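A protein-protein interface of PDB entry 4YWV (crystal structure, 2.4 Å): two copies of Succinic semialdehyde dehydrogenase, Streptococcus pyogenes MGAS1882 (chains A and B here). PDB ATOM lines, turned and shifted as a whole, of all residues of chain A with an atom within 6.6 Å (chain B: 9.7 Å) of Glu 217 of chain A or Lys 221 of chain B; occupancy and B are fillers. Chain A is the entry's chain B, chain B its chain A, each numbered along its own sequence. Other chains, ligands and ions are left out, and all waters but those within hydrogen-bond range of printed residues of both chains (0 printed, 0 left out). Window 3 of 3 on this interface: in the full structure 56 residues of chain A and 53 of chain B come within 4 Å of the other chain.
O of Ala 213 of chain B lies close to O of Gly 220 of chain A (3.5 Å).
Among the printed residues, merely in contact across the chains: Gly 220 of chain A with Ala 216 of chain B, Ala 216 of chain A with Gly 220 of chain B, Glu 209 of chain A with Leu 223 of chain B, Glu 217 of chain A with Glu 217 of chain B, Lys 221 of chain A with Glu 217 of chain B, Ala 213 of chain A with Gly 220 of chain B, Ala 213 of chain A with Leu 223 of chain B, Lys 221 of chain A with Ala 213 of chain B, Glu 217 of chain A with Lys 221 of chain B, Ala 213 of chain A with Lys 221 of chain B, Glu 217 of chain A with Gly 220 of chain B, Gly 220 of chain A with Glu 217 of chain B and Gly 212 of chain A with Leu 223 of chain B.
Of the printed residues of chain B, Glu 209 of chain A touches Leu 223. Of chain B, only Gly 220 (3.6 Å), Lys 221 (3.7 Å) and Leu 223 (3.7 Å) come within 4 Å of Ala 213 of chain A. Of chain B, only Gly 220 comes within 4 Å of Ala 216 of chain A. Of chain B, only Glu 217 (3.6 Å), Gly 220 (3.7 Å) and Lys 221 (3.7 Å) come within 4 Å of Glu 217 of chain A. Ala 219 of chain A touches none of the printed residues of chain B. Of the printed residues of chain B, Lys 221 of chain A touches Ala 213 and Glu 217. Of the printed residues of chain A, Ala 213 of chain B touches Gly 220 (3.5 Å) and Lys 221 (3.7 Å). Of chain A, only Ala 213 (3.7 Å) and Glu 217 (3.7 Å) come within 4 Å of Lys 221 of chain B. Of the printed residues of chain A, Leu 223 of chain B touches Glu 209, Gly 212 and Ala 213. The nearest residue of chain A that does not touch Lys 221 of chain B is Ala 216 of chain A (4.8 Å).
Printed residues of chain B that touch a printed residue of chain A: Ala 213, Ala 216, Glu 217, Gly 220, Lys 221 and Leu 223. Hydrophobic or aromatic side chains of chain B within 4 Å of the printed part of chain A: Ala 213, Ala 216 and Leu 223. Of the 13 printed residues of chain A, 7 touch a printed residue of chain B. Hydrophobic or aromatic side chains of chain A within 4 Å of the printed part of chain B: Ala 213 and Ala 216. Along chain A the printed residues that touch a printed residue of chain B span positions 209 to 221. Among the printed residues, 14 pairs touch across the chains. Among the printed residues, no Asp or Glu carboxylate lies within 4 Å of a Lys or Arg side-chain nitrogen of the other chain.
Ala 216 of chain A touches Gly 220 of chain B, and with the chains exchanged Gly 220 of chain A touches Ala 216 of chain B. Glu 217 of chain B touches its own counterpart, Glu 217 of chain A. Glu 217 of chain A touches Gly 220 of chain B, and with the chains exchanged Gly 220 of chain A touches Glu 217 of chain B. Glu 217 of chain A touches Lys 221 of chain B, and with the chains exchanged Lys 221 of chain A touches Glu 217 of chain B. Positions printed for both chains: 212, 213, 214, 215, 216, 217, 218, 219, 220, 221 and 222. Of the 14 pairs that touch across the chains among the printed residues, 11 have their exchanged pair printed and touching as well.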
ATOM      1  N   GLU A 209       9.379   5.131  22.878  1.00  0.00           N
ATOM      2  CA  GLU A 209       8.994   5.910  21.714  1.00  0.00           C
ATOM      3  C   GLU A 209       7.845   5.248  20.948  1.00  0.00           C
ATOM      4  O   GLU A 209       6.949   5.927  20.449  1.00  0.00           O
ATOM      5  CB  GLU A 209      10.207   6.077  20.799  1.00  0.00           C
ATOM      6  CG  GLU A 209      10.025   7.130  19.731  1.00  0.00           C
ATOM      7  CD  GLU A 209      11.234   7.263  18.823  1.00  0.00           C
ATOM      8  OE1 GLU A 209      12.350   7.509  19.339  1.00  0.00           O
ATOM      9  OE2 GLU A 209      11.059   7.124  17.590  1.00  0.00           O
ATOM     10  N   GLY A 211       5.547   3.183  22.198  1.00  0.00           N
ATOM     11  CA  GLY A 211       4.358   3.352  23.006  1.00  0.00           C
ATOM     12  C   GLY A 211       3.778   4.742  22.848  1.00  0.00           C
ATOM     13  O   GLY A 211       2.608   4.895  22.485  1.00  0.00           O
ATOM     14  N   GLY A 212       4.600   5.755  23.113  1.00  0.00           N
ATOM     15  CA  GLY A 212       4.152   7.132  22.991  1.00  0.00           C
ATOM     16  C   GLY A 212       3.485   7.398  21.654  1.00  0.00           C
ATOM     17  O   GLY A 212       2.465   8.081  21.587  1.00  0.00           O
ATOM     18  N   ALA A 213       4.065   6.846  20.593  1.00  0.00           N
ATOM     19  CA  ALA A 213       3.550   7.005  19.239  1.00  0.00           C
ATOM     20  C   ALA A 213       2.170   6.382  19.086  1.00  0.00           C
ATOM     21  O   ALA A 213       1.272   6.991  18.507  1.00  0.00           O
ATOM     22  CB  ALA A 213       4.519   6.384  18.237  1.00  0.00           C
ATOM     23  N   SER A 214       1.998   5.167  19.598  1.00  0.00           N
ATOM     24  CA  SER A 214       0.706   4.495  19.503  1.00  0.00           C
ATOM     25  C   SER A 214      -0.342   5.257  20.285  1.00  0.00           C
ATOM     26  O   SER A 214      -1.407   5.587  19.767  1.00  0.00           O
ATOM     27  CB  SER A 214       0.782   3.075  20.063  1.00  0.00           C
ATOM     28  OG  SER A 214       1.731   2.297  19.359  1.00  0.00           O
ATOM     29  N   ILE A 215      -0.031   5.532  21.544  1.00  0.00           N
ATOM     30  CA  ILE A 215      -0.960   6.227  22.421  1.00  0.00           C
ATOM     31  C   ILE A 215      -1.304   7.639  21.966  1.00  0.00           C
ATOM     32  O   ILE A 215      -2.464   8.048  22.041  1.00  0.00           O
ATOM     33  CB  ILE A 215      -0.412   6.271  23.867  1.00  0.00           C
ATOM     34  CG1 ILE A 215      -0.076   4.849  24.336  1.00  0.00           C
ATOM     35  CG2 ILE A 215      -1.417   6.935  24.797  1.00  0.00           C
ATOM     36  CD1 ILE A 215      -1.191   3.858  24.182  1.00  0.00           C
ATOM     37  N   ALA A 216      -0.308   8.383  21.490  1.00  0.00           N
ATOM     38  CA  ALA A 216      -0.548   9.754  21.046  1.00  0.00           C
ATOM     39  C   ALA A 216      -1.419   9.751  19.800  1.00  0.00           C
ATOM     40  O   ALA A 216      -2.345  10.553  19.662  1.00  0.00           O
ATOM     41  CB  ALA A 216       0.775  10.457  20.770  1.00  0.00           C
ATOM     42  N   GLU A 217      -1.126   8.829  18.895  1.00  0.00           N
ATOM     43  CA  GLU A 217      -1.895   8.720  17.668  1.00  0.00           C
ATOM     44  C   GLU A 217      -3.372   8.447  17.963  1.00  0.00           C
ATOM     45  O   GLU A 217      -4.250   9.093  17.393  1.00  0.00           O
ATOM     46  CB  GLU A 217      -1.309   7.614  16.791  1.00  0.00           C
ATOM     47  CG  GLU A 217      -2.094   7.332  15.535  1.00  0.00           C
ATOM     48  CD  GLU A 217      -1.386   6.346  14.629  1.00  0.00           C
ATOM     49  OE1 GLU A 217      -0.470   5.650  15.125  1.00  0.00           O
ATOM     50  OE2 GLU A 217      -1.749   6.261  13.431  1.00  0.00           O
ATOM     51  N   GLU A 218      -3.651   7.499  18.850  1.00  0.00           N
ATOM     52  CA  GLU A 218      -5.036   7.188  19.196  1.00  0.00           C
ATOM     53  C   GLU A 218      -5.654   8.427  19.834  1.00  0.00           C
ATOM     54  O   GLU A 218      -6.816   8.758  19.586  1.00  0.00           O
ATOM     55  CB  GLU A 218      -5.097   5.998  20.166  1.00  0.00           C
ATOM     56  CG  GLU A 218      -4.425   4.743  19.612  1.00  0.00           C
ATOM     57  CD  GLU A 218      -4.348   3.587  20.605  1.00  0.00           C
ATOM     58  OE1 GLU A 218      -3.897   3.800  21.752  1.00  0.00           O
ATOM     59  OE2 GLU A 218      -4.720   2.454  20.225  1.00  0.00           O
ATOM     60  N   ALA A 219      -4.863   9.122  20.643  1.00  0.00           N
ATOM     61  CA  ALA A 219      -5.333  10.329  21.305  1.00  0.00           C
ATOM     62  C   ALA A 219      -5.672  11.411  20.273  1.00  0.00           C
ATOM     63  O   ALA A 219      -6.670  12.127  20.402  1.00  0.00           O
ATOM     64  CB  ALA A 219      -4.261  10.838  22.275  1.00  0.00           C
ATOM     65  N   GLY A 220      -4.830  11.532  19.253  1.00  0.00           N
ATOM     66  CA  GLY A 220      -5.067  12.528  18.226  1.00  0.00           C
ATOM     67  C   GLY A 220      -6.361  12.272  17.482  1.00  0.00           C
ATOM     68  O   GLY A 220      -7.126  13.192  17.206  1.00  0.00           O
ATOM     69  N   LYS A 221      -6.601  11.010  17.156  1.00  0.00           N
ATOM     70  CA  LYS A 221      -7.807  10.602  16.447  1.00  0.00           C
ATOM     71  C   LYS A 221      -9.070  10.872  17.279  1.00  0.00           C
ATOM     72  O   LYS A 221     -10.164  11.013  16.734  1.00  0.00           O
ATOM     73  CB  LYS A 221      -7.704   9.109  16.098  1.00  0.00           C
ATOM     74  CG  LYS A 221      -9.008   8.449  15.674  1.00  0.00           C
ATOM     75  CD  LYS A 221      -8.823   6.949  15.448  1.00  0.00           C
ATOM     76  CE  LYS A 221     -10.167   6.257  15.222  1.00  0.00           C
ATOM     77  NZ  LYS A 221     -11.093   6.428  16.392  1.00  0.00           N
ATOM     78  N   ASN A 222      -8.920  10.951  18.597  1.00  0.00           N
ATOM     79  CA  ASN A 222     -10.062  11.196  19.462  1.00  0.00           C
ATOM     80  C   ASN A 222     -10.071  12.613  20.031  1.00  0.00           C
ATOM     81  O   ASN A 222     -10.831  12.928  20.949  1.00  0.00           O
ATOM     82  CB  ASN A 222     -10.099  10.148  20.580  1.00  0.00           C
ATOM     83  CG  ASN A 222     -10.488   8.762  20.066  1.00  0.00           C
ATOM     84  OD1 ASN A 222     -11.648   8.510  19.743  1.00  0.00           O
ATOM     85  ND2 ASN A 222      -9.511   7.868  19.975  1.00  0.00           N
ATOM     86  N   ASP B 189      -2.373  15.136   1.570  1.00  0.00           N
ATOM     87  CA  ASP B 189      -1.385  14.069   1.513  1.00  0.00           C
ATOM     88  C   ASP B 189      -0.026  14.691   1.879  1.00  0.00           C
ATOM     89  O   ASP B 189       0.734  14.144   2.683  1.00  0.00           O
ATOM     90  CB  ASP B 189      -1.318  13.509   0.095  1.00  0.00           C
ATOM     91  CG  ASP B 189      -1.342  11.996   0.062  1.00  0.00           C
ATOM     92  OD1 ASP B 189      -2.424  11.405   0.315  1.00  0.00           O
ATOM     93  OD2 ASP B 189      -0.274  11.405  -0.217  1.00  0.00           O
ATOM     94  N   SER B 192       0.350  15.608   5.406  1.00  0.00           N
ATOM     95  CA  SER B 192       0.733  14.463   6.199  1.00  0.00           C
ATOM     96  C   SER B 192       2.242  14.249   6.159  1.00  0.00           C
ATOM     97  O   SER B 192       2.835  13.858   7.162  1.00  0.00           O
ATOM     98  CB  SER B 192       0.015  13.220   5.689  1.00  0.00           C
ATOM     99  OG  SER B 192       0.291  12.124   6.534  1.00  0.00           O
ATOM    100  N   GLN B 193       2.857  14.500   5.002  1.00  0.00           N
ATOM    101  CA  GLN B 193       4.311  14.350   4.837  1.00  0.00           C
ATOM    102  C   GLN B 193       5.063  15.427   5.621  1.00  0.00           C
ATOM    103  O   GLN B 193       6.193  15.222   6.066  1.00  0.00           O
ATOM    104  CB  GLN B 193       4.700  14.482   3.370  1.00  0.00           C
ATOM    105  CG  GLN B 193       4.162  13.413   2.454  1.00  0.00           C
ATOM    106  CD  GLN B 193       4.277  13.826   0.998  1.00  0.00           C
ATOM    107  OE1 GLN B 193       5.321  14.325   0.567  1.00  0.00           O
ATOM    108  NE2 GLN B 193       3.203  13.623   0.232  1.00  0.00           N
ATOM    109  N   ILE B 195       3.903  16.870   8.461  1.00  0.00           N
ATOM    110  CA  ILE B 195       3.804  16.508   9.867  1.00  0.00           C
ATOM    111  C   ILE B 195       4.779  15.390  10.207  1.00  0.00           C
ATOM    112  O   ILE B 195       5.206  15.257  11.347  1.00  0.00           O
ATOM    113  CB  ILE B 195       2.389  16.057  10.212  1.00  0.00           C
ATOM    114  CG1 ILE B 195       1.437  17.237  10.040  1.00  0.00           C
ATOM    115  CG2 ILE B 195       2.344  15.488  11.632  1.00  0.00           C
ATOM    116  CD1 ILE B 195      -0.027  16.830  10.024  1.00  0.00           C
ATOM    117  N   ALA B 196       5.138  14.594   9.207  1.00  0.00           N
ATOM    118  CA  ALA B 196       6.067  13.496   9.412  1.00  0.00           C
ATOM    119  C   ALA B 196       7.520  13.946   9.298  1.00  0.00           C
ATOM    120  O   ALA B 196       8.424  13.225   9.704  1.00  0.00           O
ATOM    121  CB  ALA B 196       5.788  12.390   8.408  1.00  0.00           C
ATOM    122  N   ASP B 197       7.746  15.136   8.750  1.00  0.00           N
ATOM    123  CA  ASP B 197       9.101  15.671   8.591  1.00  0.00           C
ATOM    124  C   ASP B 197       9.748  16.019   9.944  1.00  0.00           C
ATOM    125  O   ASP B 197       9.130  16.667  10.787  1.00  0.00           O
ATOM    126  CB  ASP B 197       9.042  16.922   7.716  1.00  0.00           C
ATOM    127  CG  ASP B 197      10.383  17.271   7.094  1.00  0.00           C
ATOM    128  OD1 ASP B 197      10.676  16.756   5.988  1.00  0.00           O
ATOM    129  OD2 ASP B 197      11.137  18.056   7.716  1.00  0.00           O
ATOM    130  N   GLY B 212      -9.446  18.066  11.845  1.00  0.00           N
ATOM    131  CA  GLY B 212      -8.630  18.189  13.038  1.00  0.00           C
ATOM    132  C   GLY B 212      -8.189  16.846  13.584  1.00  0.00           C
ATOM    133  O   GLY B 212      -7.025  16.663  13.940  1.00  0.00           O
ATOM    134  N   ALA B 213      -9.113  15.894  13.651  1.00  0.00           N
ATOM    135  CA  ALA B 213      -8.784  14.579  14.171  1.00  0.00           C
ATOM    136  C   ALA B 213      -7.749  13.904  13.281  1.00  0.00           C
ATOM    137  O   ALA B 213      -6.793  13.295  13.765  1.00  0.00           O
ATOM    138  CB  ALA B 213     -10.038  13.726  14.261  1.00  0.00           C
ATOM    139  N   SER B 214      -7.935  14.020  11.975  1.00  0.00           N
ATOM    140  CA  SER B 214      -7.011  13.409  11.036  1.00  0.00           C
ATOM    141  C   SER B 214      -5.596  13.971  11.191  1.00  0.00           C
ATOM    142  O   SER B 214      -4.620  13.227  11.230  1.00  0.00           O
ATOM    143  CB  SER B 214      -7.513  13.620   9.608  1.00  0.00           C
ATOM    144  OG  SER B 214      -6.523  13.238   8.672  1.00  0.00           O
ATOM    145  N   ILE B 215      -5.480  15.286  11.288  1.00  0.00           N
ATOM    146  CA  ILE B 215      -4.170  15.897  11.437  1.00  0.00           C
ATOM    147  C   ILE B 215      -3.545  15.540  12.791  1.00  0.00           C
ATOM    148  O   ILE B 215      -2.351  15.267  12.871  1.00  0.00           O
ATOM    149  CB  ILE B 215      -4.267  17.446  11.264  1.00  0.00           C
ATOM    150  CG1 ILE B 215      -4.326  17.802   9.774  1.00  0.00           C
ATOM    151  CG2 ILE B 215      -3.070  18.145  11.914  1.00  0.00           C
ATOM    152  CD1 ILE B 215      -5.423  17.096   9.010  1.00  0.00           C
ATOM    153  N   ALA B 216      -4.347  15.532  13.852  1.00  0.00           N
ATOM    154  CA  ALA B 216      -3.825  15.213  15.183  1.00  0.00           C
ATOM    155  C   ALA B 216      -3.339  13.773  15.224  1.00  0.00           C
ATOM    156  O   ALA B 216      -2.351  13.451  15.878  1.00  0.00           O
ATOM    157  CB  ALA B 216      -4.897  15.440  16.244  1.00  0.00           C
ATOM    158  N   GLU B 217      -4.041  12.907  14.514  1.00  0.00           N
ATOM    159  CA  GLU B 217      -3.666  11.511  14.454  1.00  0.00           C
ATOM    160  C   GLU B 217      -2.281  11.380  13.816  1.00  0.00           C
ATOM    161  O   GLU B 217      -1.436  10.620  14.284  1.00  0.00           O
ATOM    162  CB  GLU B 217      -4.707  10.750  13.647  1.00  0.00           C
ATOM    163  CG  GLU B 217      -4.371   9.303  13.398  1.00  0.00           C
ATOM    164  CD  GLU B 217      -5.569   8.516  12.910  1.00  0.00           C
ATOM    165  OE1 GLU B 217      -6.243   8.977  11.956  1.00  0.00           O
ATOM    166  OE2 GLU B 217      -5.832   7.435  13.484  1.00  0.00           O
ATOM    167  N   GLU B 218      -2.043  12.136  12.754  1.00  0.00           N
ATOM    168  CA  GLU B 218      -0.754  12.091  12.078  1.00  0.00           C
ATOM    169  C   GLU B 218       0.304  12.706  12.980  1.00  0.00           C
ATOM    170  O   GLU B 218       1.447  12.264  13.006  1.00  0.00           O
ATOM    171  CB  GLU B 218      -0.835  12.843  10.746  1.00  0.00           C
ATOM    172  CG  GLU B 218      -1.884  12.255   9.797  1.00  0.00           C
ATOM    173  CD  GLU B 218      -2.195  13.156   8.606  1.00  0.00           C
ATOM    174  OE1 GLU B 218      -2.442  14.365   8.820  1.00  0.00           O
ATOM    175  OE2 GLU B 218      -2.211  12.653   7.460  1.00  0.00           O
ATOM    176  N   ALA B 219      -0.085  13.726  13.729  1.00  0.00           N
ATOM    177  CA  ALA B 219       0.846  14.387  14.640  1.00  0.00           C
ATOM    178  C   ALA B 219       1.264  13.440  15.768  1.00  0.00           C
ATOM    179  O   ALA B 219       2.449  13.306  16.069  1.00  0.00           O
ATOM    180  CB  ALA B 219       0.211  15.645  15.222  1.00  0.00           C
ATOM    181  N   GLY B 220       0.285  12.787  16.389  1.00  0.00           N
ATOM    182  CA  GLY B 220       0.583  11.869  17.471  1.00  0.00           C
ATOM    183  C   GLY B 220       1.474  10.727  17.029  1.00  0.00           C
ATOM    184  O   GLY B 220       2.401  10.336  17.737  1.00  0.00           O
ATOM    185  N   LYS B 221       1.193  10.179  15.852  1.00  0.00           N
ATOM    186  CA  LYS B 221       1.988   9.082  15.332  1.00  0.00           C
ATOM    187  C   LYS B 221       3.443   9.514  15.216  1.00  0.00           C
ATOM    188  O   LYS B 221       4.355   8.701  15.381  1.00  0.00           O
ATOM    189  CB  LYS B 221       1.468   8.652  13.956  1.00  0.00           C
ATOM    190  CG  LYS B 221       2.207   7.455  13.368  1.00  0.00           C
ATOM    191  CD  LYS B 221       1.679   7.064  11.997  1.00  0.00           C
ATOM    192  CE  LYS B 221       2.021   8.111  10.944  1.00  0.00           C
ATOM    193  NZ  LYS B 221       1.602   7.698   9.570  1.00  0.00           N
ATOM    194  N   ASN B 222       3.658  10.799  14.949  1.00  0.00           N
ATOM    195  CA  ASN B 222       5.005  11.339  14.786  1.00  0.00           C
ATOM    196  C   ASN B 222       5.566  12.071  15.991  1.00  0.00           C
ATOM    197  O   ASN B 222       6.580  12.755  15.876  1.00  0.00           O
ATOM    198  CB  ASN B 222       5.040  12.259  13.569  1.00  0.00           C
ATOM    199  CG  ASN B 222       4.940  11.495  12.264  1.00  0.00           C
ATOM    200  OD1 ASN B 222       5.910  10.873  11.824  1.00  0.00           O
ATOM    201  ND2 ASN B 222       3.762  11.521  11.644  1.00  0.00           N
ATOM    202  N   LEU B 223       4.909  11.927  17.138  1.00  0.00           N
ATOM    203  CA  LEU B 223       5.343  12.564  18.388  1.00  0.00           C
ATOM    204  C   LEU B 223       5.462  14.084  18.314  1.00  0.00           C
ATOM    205  O   LEU B 223       6.428  14.655  18.806  1.00  0.00           O
ATOM    206  CB  LEU B 223       6.689  11.979  18.824  1.00  0.00           C
ATOM    207  CG  LEU B 223       6.677  10.456  18.935  1.00  0.00           C
ATOM    208  CD1 LEU B 223       8.092   9.946  19.099  1.00  0.00           C
ATOM    209  CD2 LEU B 223       5.793  10.033  20.098  1.00  0.00           C
ATOM    210  N   LYS B 224       4.481  14.741  17.712  1.00  0.00           N
ATOM    211  CA  LYS B 224       4.526  16.192  17.587  1.00  0.00           C
ATOM    212  C   LYS B 224       3.418  16.837  18.403  1.00  0.00           C
ATOM    213  O   LYS B 224       2.262  16.424  18.331  1.00  0.00           O
ATOM    214  CB  LYS B 224       4.371  16.587  16.121  1.00  0.00           C
ATOM    215  CG  LYS B 224       5.325  15.871  15.156  1.00  0.00           C
ATOM    216  CD  LYS B 224       6.759  16.369  15.292  1.00  0.00           C
ATOM    217  CE  LYS B 224       7.691  15.674  14.311  1.00  0.00           C
ATOM    218  NZ  LYS B 224       7.344  15.959  12.895  1.00  0.00           N
ATOM    219  N   LYS B 225       3.766  17.847  19.188  1.00  0.00           N
ATOM    220  CA  LYS B 225       2.768  18.534  19.995  1.00  0.00           C
ATOM    221  C   LYS B 225       1.748  19.225  19.093  1.00  0.00           C
ATOM    222  O   LYS B 225       2.065  19.641  17.973  1.00  0.00           O
ATOM    223  CB  LYS B 225       3.433  19.577  20.903  1.00  0.00           C
ATOM    224  CG  LYS B 225       2.437  20.384  21.711  1.00  0.00           C
ATOM    225  CD  LYS B 225       3.090  21.213  22.800  1.00  0.00           C
ATOM    226  CE  LYS B 225       2.023  21.990  23.576  1.00  0.00           C
ATOM    227  NZ  LYS B 225       2.572  22.657  24.798  1.00  0.00           N
ATOM    228  N   THR B 226       0.518  19.339  19.575  1.00  0.00           N
ATOM    229  CA  THR B 226      -0.509  20.005  18.800  1.00  0.00           C
ATOM    230  C   THR B 226      -1.414  20.828  19.692  1.00  0.00           C
ATOM    231  O   THR B 226      -1.376  20.711  20.915  1.00  0.00           O
ATOM    232  CB  THR B 226      -1.404  19.009  18.056  1.00  0.00           C
ATOM    233  OG1 THR B 226      -2.133  18.228  19.011  1.00  0.00           O
ATOM    234  CG2 THR B 226      -0.578  18.103  17.174  1.00  0.00           C
ATOM    235  N   TYR B 434      -8.278  21.582  22.357  1.00  0.00           N
ATOM    236  CA  TYR B 434      -7.475  21.785  23.548  1.00  0.00           C
ATOM    237  C   TYR B 434      -6.350  22.741  23.183  1.00  0.00           C
ATOM    238  O   TYR B 434      -6.041  22.932  22.002  1.00  0.00           O
ATOM    239  CB  TYR B 434      -6.918  20.445  24.056  1.00  0.00           C
ATOM    240  CG  TYR B 434      -6.228  19.618  22.992  1.00  0.00           C
ATOM    241  CD1 TYR B 434      -4.930  19.931  22.563  1.00  0.00           C
ATOM    242  CD2 TYR B 434      -6.884  18.552  22.383  1.00  0.00           C
ATOM    243  CE1 TYR B 434      -4.307  19.201  21.549  1.00  0.00           C
ATOM    244  CE2 TYR B 434      -6.271  17.815  21.371  1.00  0.00           C
ATOM    245  CZ  TYR B 434      -4.987  18.146  20.961  1.00  0.00           C
ATOM    246  OH  TYR B 434      -4.395  17.419  19.962  1.00  0.00           O
